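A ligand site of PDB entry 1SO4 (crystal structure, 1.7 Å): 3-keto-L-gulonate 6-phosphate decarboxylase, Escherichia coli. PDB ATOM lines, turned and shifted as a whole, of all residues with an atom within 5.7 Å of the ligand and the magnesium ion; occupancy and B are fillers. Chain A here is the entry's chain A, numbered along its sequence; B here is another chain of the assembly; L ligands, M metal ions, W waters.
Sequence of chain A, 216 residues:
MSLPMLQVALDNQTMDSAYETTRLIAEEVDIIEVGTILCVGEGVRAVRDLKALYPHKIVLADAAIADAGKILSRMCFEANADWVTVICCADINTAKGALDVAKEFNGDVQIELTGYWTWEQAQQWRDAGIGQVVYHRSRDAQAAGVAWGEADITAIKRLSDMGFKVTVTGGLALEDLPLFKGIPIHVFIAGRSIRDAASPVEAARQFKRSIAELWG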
ATOM      1  N   ALA A   9       3.396 -19.919 -15.429  1.00  0.00           N
ATOM      2  CA  ALA A   9       4.700 -19.274 -15.704  1.00  0.00           C
ATOM      3  C   ALA A   9       4.490 -17.782 -15.813  1.00  0.00           C
ATOM      4  O   ALA A   9       3.763 -17.294 -16.718  1.00  0.00           O
ATOM      5  CB  ALA A   9       5.362 -19.822 -16.962  1.00  0.00           C
ATOM      6  N   ASP A  11       6.201 -15.172 -17.130  1.00  0.00           N
ATOM      7  CA  ASP A  11       7.197 -14.701 -18.076  1.00  0.00           C
ATOM      8  C   ASP A  11       6.877 -13.267 -18.377  1.00  0.00           C
ATOM      9  O   ASP A  11       6.484 -12.892 -19.494  1.00  0.00           O
ATOM     10  CB  ASP A  11       7.224 -15.587 -19.314  1.00  0.00           C
ATOM     11  CG  ASP A  11       7.830 -16.907 -19.034  1.00  0.00           C
ATOM     12  OD1 ASP A  11       8.922 -16.926 -18.369  1.00  0.00           O
ATOM     13  OD2 ASP A  11       7.307 -17.994 -19.422  1.00  0.00           O
ATOM     14  N   GLU A  33       5.523 -19.784 -10.932  1.00  0.00           N
ATOM     15  CA  GLU A  33       6.847 -19.703 -11.496  1.00  0.00           C
ATOM     16  C   GLU A  33       7.225 -18.243 -11.742  1.00  0.00           C
ATOM     17  O   GLU A  33       6.515 -17.463 -12.456  1.00  0.00           O
ATOM     18  CB  GLU A  33       6.913 -20.488 -12.813  1.00  0.00           C
ATOM     19  CG  GLU A  33       8.018 -20.022 -13.764  1.00  0.00           C
ATOM     20  CD  GLU A  33       8.173 -20.810 -15.028  1.00  0.00           C
ATOM     21  OE1 GLU A  33       7.577 -21.883 -15.146  1.00  0.00           O
ATOM     22  OE2 GLU A  33       8.880 -20.286 -15.933  1.00  0.00           O
ATOM     23  N   GLY A  35       9.323 -16.676 -14.049  1.00  0.00           N
ATOM     24  CA  GLY A  35       9.912 -17.057 -15.313  1.00  0.00           C
ATOM     25  C   GLY A  35      11.307 -16.529 -15.494  1.00  0.00           C
ATOM     26  O   GLY A  35      11.682 -15.580 -14.861  1.00  0.00           O
ATOM     27  N   THR A  36      12.066 -17.124 -16.399  1.00  0.00           N
ATOM     28  CA  THR A  36      13.393 -16.621 -16.656  1.00  0.00           C
ATOM     29  C   THR A  36      13.364 -15.148 -17.040  1.00  0.00           C
ATOM     30  O   THR A  36      14.221 -14.381 -16.612  1.00  0.00           O
ATOM     31  CB  THR A  36      14.046 -17.425 -17.754  1.00  0.00           C
ATOM     32  OG1 THR A  36      13.847 -18.820 -17.502  1.00  0.00           O
ATOM     33  CG2 THR A  36      15.523 -17.204 -17.746  1.00  0.00           C
ATOM     34  N   ASP A  62      12.677 -19.943 -12.247  1.00  0.00           N
ATOM     35  CA  ASP A  62      13.132 -20.512 -13.501  1.00  0.00           C
ATOM     36  C   ASP A  62      14.412 -19.786 -13.944  1.00  0.00           C
ATOM     37  O   ASP A  62      14.468 -19.110 -14.961  1.00  0.00           O
ATOM     38  CB  ASP A  62      12.029 -20.494 -14.572  1.00  0.00           C
ATOM     39  CG  ASP A  62      12.325 -21.424 -15.729  1.00  0.00           C
ATOM     40  OD1 ASP A  62      13.406 -22.102 -15.731  1.00  0.00           O
ATOM     41  OD2 ASP A  62      11.618 -21.424 -16.754  1.00  0.00           O
ATOM     42  N   GLU A 112      16.281 -28.518 -16.493  1.00  0.00           N
ATOM     43  CA  GLU A 112      15.504 -28.029 -17.626  1.00  0.00           C
ATOM     44  C   GLU A 112      16.027 -28.615 -18.921  1.00  0.00           C
ATOM     45  O   GLU A 112      17.179 -28.381 -19.306  1.00  0.00           O
ATOM     46  CB  GLU A 112      15.629 -26.538 -17.653  1.00  0.00           C
ATOM     47  CG  GLU A 112      14.607 -25.861 -18.498  1.00  0.00           C
ATOM     48  CD  GLU A 112      13.908 -24.746 -17.725  1.00  0.00           C
ATOM     49  OE1 GLU A 112      14.478 -23.642 -17.784  1.00  0.00           O
ATOM     50  OE2 GLU A 112      12.841 -25.005 -17.066  1.00  0.00           O
ATOM     51  N   THR A 114      15.767 -28.393 -22.374  1.00  0.00           N
ATOM     52  CA  THR A 114      15.375 -27.458 -23.419  1.00  0.00           C
ATOM     53  C   THR A 114      16.541 -27.532 -24.378  1.00  0.00           C
ATOM     54  O   THR A 114      17.682 -27.270 -23.975  1.00  0.00           O
ATOM     55  CB  THR A 114      15.239 -26.002 -22.918  1.00  0.00           C
ATOM     56  OG1 THR A 114      14.316 -25.885 -21.813  1.00  0.00           O
ATOM     57  CG2 THR A 114      14.588 -25.183 -24.003  1.00  0.00           C
ATOM     58  N   HIS A 136      10.703 -29.616 -21.931  1.00  0.00           N
ATOM     59  CA  HIS A 136      10.249 -28.408 -22.649  1.00  0.00           C
ATOM     60  C   HIS A 136      10.243 -28.598 -24.119  1.00  0.00           C
ATOM     61  O   HIS A 136      11.244 -29.082 -24.689  1.00  0.00           O
ATOM     62  CB  HIS A 136      11.265 -27.318 -22.529  1.00  0.00           C
ATOM     63  CG  HIS A 136      11.232 -26.531 -21.286  1.00  0.00           C
ATOM     64  ND1 HIS A 136      10.886 -25.201 -21.288  1.00  0.00           N
ATOM     65  CD2 HIS A 136      11.614 -26.833 -20.022  1.00  0.00           C
ATOM     66  CE1 HIS A 136      11.015 -24.726 -20.065  1.00  0.00           C
ATOM     67  NE2 HIS A 136      11.454 -25.698 -19.277  1.00  0.00           N
ATOM     68  N   SER A 138      10.885 -25.896 -26.573  1.00  0.00           N
ATOM     69  CA  SER A 138      11.420 -24.557 -26.577  1.00  0.00           C
ATOM     70  C   SER A 138      10.422 -23.599 -27.264  1.00  0.00           C
ATOM     71  O   SER A 138       9.865 -23.930 -28.312  1.00  0.00           O
ATOM     72  CB  SER A 138      12.745 -24.524 -27.380  1.00  0.00           C
ATOM     73  OG  SER A 138      13.036 -23.251 -27.913  1.00  0.00           O
ATOM     74  N   ARG A 139      10.224 -22.441 -26.670  1.00  0.00           N
ATOM     75  CA  ARG A 139       9.411 -21.378 -27.287  1.00  0.00           C
ATOM     76  C   ARG A 139       9.880 -21.044 -28.686  1.00  0.00           C
ATOM     77  O   ARG A 139       9.091 -20.804 -29.595  1.00  0.00           O
ATOM     78  CB  ARG A 139       9.477 -20.108 -26.428  1.00  0.00           C
ATOM     79  CG  ARG A 139       8.752 -18.927 -26.994  1.00  0.00           C
ATOM     80  CD  ARG A 139       9.049 -17.648 -26.253  1.00  0.00           C
ATOM     81  NE  ARG A 139       8.706 -17.707 -24.832  1.00  0.00           N
ATOM     82  CZ  ARG A 139       7.645 -17.146 -24.269  1.00  0.00           C
ATOM     83  NH1 ARG A 139       6.834 -16.377 -24.966  1.00  0.00           N
ATOM     84  NH2 ARG A 139       7.434 -17.285 -22.948  1.00  0.00           N
ATOM     85  N   GLN A 142       9.027 -23.908 -31.046  1.00  0.00           N
ATOM     86  CA  GLN A 142       7.604 -23.760 -31.350  1.00  0.00           C
ATOM     87  C   GLN A 142       7.384 -22.689 -32.399  1.00  0.00           C
ATOM     88  O   GLN A 142       6.622 -22.889 -33.337  1.00  0.00           O
ATOM     89  CB  GLN A 142       6.855 -23.390 -30.075  1.00  0.00           C
ATOM     90  CG  GLN A 142       5.369 -23.101 -30.270  1.00  0.00           C
ATOM     91  CD  GLN A 142       4.692 -22.568 -29.024  1.00  0.00           C
ATOM     92  OE1 GLN A 142       5.317 -22.484 -27.957  1.00  0.00           O
ATOM     93  NE2 GLN A 142       3.392 -22.228 -29.151  1.00  0.00           N
ATOM     94  N   THR A 169       6.002 -28.867 -20.462  1.00  0.00           N
ATOM     95  CA  THR A 169       5.752 -27.473 -20.803  1.00  0.00           C
ATOM     96  C   THR A 169       6.190 -27.081 -22.196  1.00  0.00           C
ATOM     97  O   THR A 169       7.101 -27.699 -22.774  1.00  0.00           O
ATOM     98  CB  THR A 169       6.457 -26.593 -19.745  1.00  0.00           C
ATOM     99  OG1 THR A 169       6.033 -25.214 -19.891  1.00  0.00           O
ATOM    100  CG2 THR A 169       7.978 -26.626 -19.938  1.00  0.00           C
ATOM    101  N   GLY A 170       5.576 -26.024 -22.716  1.00  0.00           N
ATOM    102  CA  GLY A 170       6.076 -25.393 -23.942  1.00  0.00           C
ATOM    103  C   GLY A 170       4.919 -25.100 -24.832  1.00  0.00           C
ATOM    104  O   GLY A 170       4.505 -25.921 -25.639  1.00  0.00           O
ATOM    105  N   GLY A 171       4.325 -23.944 -24.594  1.00  0.00           N
ATOM    106  CA  GLY A 171       3.193 -23.494 -25.398  1.00  0.00           C
ATOM    107  C   GLY A 171       2.007 -24.409 -25.258  1.00  0.00           C
ATOM    108  O   GLY A 171       1.191 -24.526 -26.191  1.00  0.00           O
ATOM    109  N   LEU A 172       1.879 -25.036 -24.087  1.00  0.00           N
ATOM    110  CA  LEU A 172       0.759 -25.966 -23.853  1.00  0.00           C
ATOM    111  C   LEU A 172      -0.578 -25.239 -23.924  1.00  0.00           C
ATOM    112  O   LEU A 172      -0.735 -24.161 -23.340  1.00  0.00           O
ATOM    113  CB  LEU A 172       0.867 -26.592 -22.480  1.00  0.00           C
ATOM    114  CG  LEU A 172       1.225 -28.066 -22.313  1.00  0.00           C
ATOM    115  CD1 LEU A 172       1.789 -28.776 -23.504  1.00  0.00           C
ATOM    116  CD2 LEU A 172       2.089 -28.251 -21.076  1.00  0.00           C
ATOM    117  N   ILE A 189       2.940 -27.013 -16.886  1.00  0.00           N
ATOM    118  CA  ILE A 189       3.088 -25.548 -16.912  1.00  0.00           C
ATOM    119  C   ILE A 189       2.337 -24.898 -18.078  1.00  0.00           C
ATOM    120  O   ILE A 189       2.425 -25.323 -19.212  1.00  0.00           O
ATOM    121  CB  ILE A 189       4.582 -25.138 -17.003  1.00  0.00           C
ATOM    122  CG1 ILE A 189       5.472 -25.824 -15.968  1.00  0.00           C
ATOM    123  CG2 ILE A 189       4.721 -23.594 -16.784  1.00  0.00           C
ATOM    124  CD1 ILE A 189       6.975 -25.519 -16.209  1.00  0.00           C
ATOM    125  N   ALA A 190       1.669 -23.803 -17.762  1.00  0.00           N
ATOM    126  CA  ALA A 190       1.043 -22.920 -18.744  1.00  0.00           C
ATOM    127  C   ALA A 190       1.447 -21.508 -18.412  1.00  0.00           C
ATOM    128  O   ALA A 190       1.221 -21.034 -17.287  1.00  0.00           O
ATOM    129  CB  ALA A 190      -0.436 -23.047 -18.659  1.00  0.00           C
ATOM    130  N   GLY A 191       1.990 -20.815 -19.399  1.00  0.00           N
ATOM    131  CA  GLY A 191       2.292 -19.409 -19.285  1.00  0.00           C
ATOM    132  C   GLY A 191       1.304 -18.666 -20.175  1.00  0.00           C
ATOM    133  O   GLY A 191       0.269 -18.215 -19.701  1.00  0.00           O
ATOM    134  N   ARG A 192       1.606 -18.552 -21.443  1.00  0.00           N
ATOM    135  CA  ARG A 192       0.769 -17.768 -22.361  1.00  0.00           C
ATOM    136  C   ARG A 192      -0.713 -18.186 -22.364  1.00  0.00           C
ATOM    137  O   ARG A 192      -1.585 -17.311 -22.451  1.00  0.00           O
ATOM    138  CB  ARG A 192       1.336 -17.864 -23.757  1.00  0.00           C
ATOM    139  CG  ARG A 192       2.568 -17.057 -23.945  1.00  0.00           C
ATOM    140  CD  ARG A 192       3.316 -17.435 -25.199  1.00  0.00           C
ATOM    141  NE  ARG A 192       4.005 -18.687 -25.071  1.00  0.00           N
ATOM    142  CZ  ARG A 192       4.568 -19.352 -26.073  1.00  0.00           C
ATOM    143  NH1 ARG A 192       5.209 -20.458 -25.828  1.00  0.00           N
ATOM    144  NH2 ARG A 192       4.488 -18.890 -27.320  1.00  0.00           N
ATOM    145  N   SER A 193      -0.980 -19.493 -22.303  1.00  0.00           N
ATOM    146  CA  SER A 193      -2.353 -20.050 -22.386  1.00  0.00           C
ATOM    147  C   SER A 193      -3.199 -19.629 -21.174  1.00  0.00           C
ATOM    148  O   SER A 193      -4.439 -19.672 -21.234  1.00  0.00           O
ATOM    149  CB  SER A 193      -2.267 -21.602 -22.596  1.00  0.00           C
ATOM    150  OG  SER A 193      -1.946 -22.254 -21.384  1.00  0.00           O
ATOM    151  N   ARG A 195      -2.005 -16.537 -18.951  1.00  0.00           N
ATOM    152  CA  ARG A 195      -1.830 -15.103 -18.801  1.00  0.00           C
ATOM    153  C   ARG A 195      -2.558 -14.345 -19.890  1.00  0.00           C
ATOM    154  O   ARG A 195      -3.098 -13.271 -19.632  1.00  0.00           O
ATOM    155  CB  ARG A 195      -0.349 -14.743 -18.897  1.00  0.00           C
ATOM    156  CG  ARG A 195       0.527 -15.325 -17.818  1.00  0.00           C
ATOM    157  CD  ARG A 195       1.835 -14.585 -17.677  1.00  0.00           C
ATOM    158  NE  ARG A 195       2.378 -14.275 -18.990  1.00  0.00           N
ATOM    159  CZ  ARG A 195       3.146 -15.101 -19.696  1.00  0.00           C
ATOM    160  NH1 ARG A 195       3.549 -16.262 -19.184  1.00  0.00           N
ATOM    161  NH2 ARG A 195       3.540 -14.765 -20.902  1.00  0.00           N
ATOM    162  N   ASP B  67      16.390 -19.938 -23.877  1.00  0.00           N
ATOM    163  CA  ASP B  67      15.161 -19.976 -24.673  1.00  0.00           C
ATOM    164  C   ASP B  67      14.635 -18.589 -24.659  1.00  0.00           C
ATOM    165  O   ASP B  67      15.111 -17.723 -23.884  1.00  0.00           O
ATOM    166  CB  ASP B  67      14.142 -20.910 -24.032  1.00  0.00           C
ATOM    167  CG  ASP B  67      13.001 -21.268 -24.962  1.00  0.00           C
ATOM    168  OD1 ASP B  67      13.104 -20.989 -26.178  1.00  0.00           O
ATOM    169  OD2 ASP B  67      11.936 -21.780 -24.544  1.00  0.00           O
ATOM    170  N   ALA B  68      13.634 -18.342 -25.500  1.00  0.00           N
ATOM    171  CA  ALA B  68      13.076 -17.005 -25.650  1.00  0.00           C
ATOM    172  C   ALA B  68      14.156 -15.986 -26.063  1.00  0.00           C
ATOM    173  O   ALA B  68      14.247 -14.860 -25.537  1.00  0.00           O
ATOM    174  CB  ALA B  68      12.359 -16.575 -24.374  1.00  0.00           C
HETATM  175  O1  LIG L   1       5.341 -21.693 -23.143  1.00  0.00           O
HETATM  176  P1  LIG L   1       4.432 -21.050 -22.108  1.00  0.00           P
HETATM  177  O2  LIG L   1       4.065 -19.620 -22.461  1.00  0.00           O
HETATM  178  O3  LIG L   1       3.258 -21.951 -21.679  1.00  0.00           O
HETATM  179  O4  LIG L   1       5.373 -20.840 -20.829  1.00  0.00           O
HETATM  180  C1  LIG L   1       5.931 -21.891 -20.026  1.00  0.00           C
HETATM  181  C2  LIG L   1       7.385 -22.129 -20.417  1.00  0.00           C
HETATM  182  O5  LIG L   1       7.786 -23.226 -19.598  1.00  0.00           O
HETATM  183  C3  LIG L   1       8.246 -20.886 -20.176  1.00  0.00           C
HETATM  184  O6  LIG L   1       8.153 -20.440 -18.790  1.00  0.00           O
HETATM  185  C4  LIG L   1       9.694 -21.249 -20.467  1.00  0.00           C
HETATM  186  O7  LIG L   1      10.488 -21.497 -19.455  1.00  0.00           O
HETATM  187  N1  LIG L   1      10.060 -21.278 -21.676  1.00  0.00           N
HETATM  188  O8  LIG L   1      11.450 -21.642 -21.855  1.00  0.00           O
HETATM  189 MG    MG M   1       9.852 -20.890 -17.616  1.00  0.00          MG
HETATM  190  O   HOH W   1      10.593 -19.029 -18.036  1.00  0.00           O
HETATM  191  O   HOH W   2       8.930 -22.836 -17.235  1.00  0.00           O
HETATM  192  O   HOH W   3       9.892 -18.891 -22.608  1.00  0.00           O
HETATM  193  O   HOH W   4       5.178 -17.612 -21.098  1.00  0.00           O
HETATM  194  O   HOH W   5      13.238 -21.529 -19.447  1.00  0.00           O
HETATM  195  O   HOH W   6       7.962 -21.913 -23.872  1.00  0.00           O
HETATM  196  O   HOH W   7       9.384 -24.107 -23.152  1.00  0.00           O
HETATM  197  O   HOH W   8       0.967 -21.764 -22.902  1.00  0.00           O
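N of Arg 192 lies within hydrogen-bond range of O2 of the ligand (2.9 Å). The side-chain carboxylate (OD2) of Asp 67 of chain B sits at hydrogen-bond distance from an oxygen (O8) of the ligand (2.7 Å). O6 of the ligand lies close to OD2 of Asp 11, at 2.7 Å. NE of Arg 192 lies within salt-bridge range of O2 of the ligand, at 2.8 Å. O1 of the ligand sits at hydrogen-bond distance from N of Gly 171 (2.9 Å). An oxygen (O3) of the ligand lies within hydrogen-bond range of the backbone NH (N) of Gly 191 (2.8 Å). The side-chain hydroxyl of Thr 169 lies within hydrogen-bond range of an oxygen (O5) of the ligand (2.7 Å).
The side-chain carboxylate (OD1) of Asp 67 of chain B lies within hydrogen-bond range of the side-chain hydroxyl (OG) of Ser 138 (2.9 Å). The guanidinium group (NH1) of Arg 195 lies within hydrogen-bond range of the backbone carbonyl oxygen (O) of Ala 9, at 2.7 Å. The backbone carbonyl oxygen (O) of Asp 62 lies within hydrogen-bond range of the side-chain hydroxyl (OG1) of Thr 36 (2.6 Å). The side-chain carboxylate (OD2) of Asp 67 of chain B sits at hydrogen-bond distance from the backbone NH (N) of Arg 139 (2.8 Å). The guanidinium group of Arg 139 lies within salt-bridge range of the side-chain carboxylate of Asp 11. A ring nitrogen (NE2) of His 136 lies within hydrogen-bond range of the side-chain carboxylate (OE2) of Glu 112 (2.7 Å). N of Ala 9 is in hydrogen-bond range of O of Ala 190 (3.1 Å). NH1 of Arg 192 lies within hydrogen-bond range of OE1 of Gln 142, 2.9 Å away.
Ala 9 touches the ligand. His 136 touches the ligand (CE1 to O7, 3.3 Å). Gly 170 touches the ligand (C to O1, 3.8 Å). Ile 189 touches the ligand. C of Ala 190 touches O3 of the ligand, 3.8 Å away. Within 4 Å of the ligand: Ala 9, Asp 11, Glu 33, Asp 62, His 136, Thr 169, Gly 170, Gly 171, Ile 189, Ala 190, Gly 191, Arg 192 and Asp 67 of chain B.
Two residues have an atom within 4 Å of the magnesium ion: Glu 33 and Asp 62.
The magnesium ion is bound by the side-chain carboxylate of Glu 33 (2.0 Å), the side-chain carboxylate of Asp 62 (2.0 Å), an oxygen (O7) of the ligand (2.0 Å), water W1 (2.0 Å), an oxygen (O6) of the ligand (2.1 Å) and water W2 (2.2 Å).
Water W2 lies within hydrogen-bond range of an oxygen (O5) of the ligand (2.7 Å) and the side-chain carboxylate (OE1) of Glu 33 (2.7 Å). Water W3 bridges a nitrogen (N1) of the ligand (2.6 Å) and the guanidinium group of Arg 139 (2.8 Å). Water W8 lies within hydrogen-bond range of O3 of the ligand, O of Leu 172 and N of Ser 193. Water W4 lies within hydrogen-bond range of O2 of the ligand, OD2 of Asp 11, NH1 of Arg 195 and NH2 of Arg 139. Water W5 lies within hydrogen-bond range of OE1 of Glu 112 (3.0 Å), O8 of the ligand (3.0 Å) and OG1 of Thr 36 (3.4 Å). Water W7 bridges a ring nitrogen (ND1) of His 136 and a nitrogen (N1) of the ligand.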
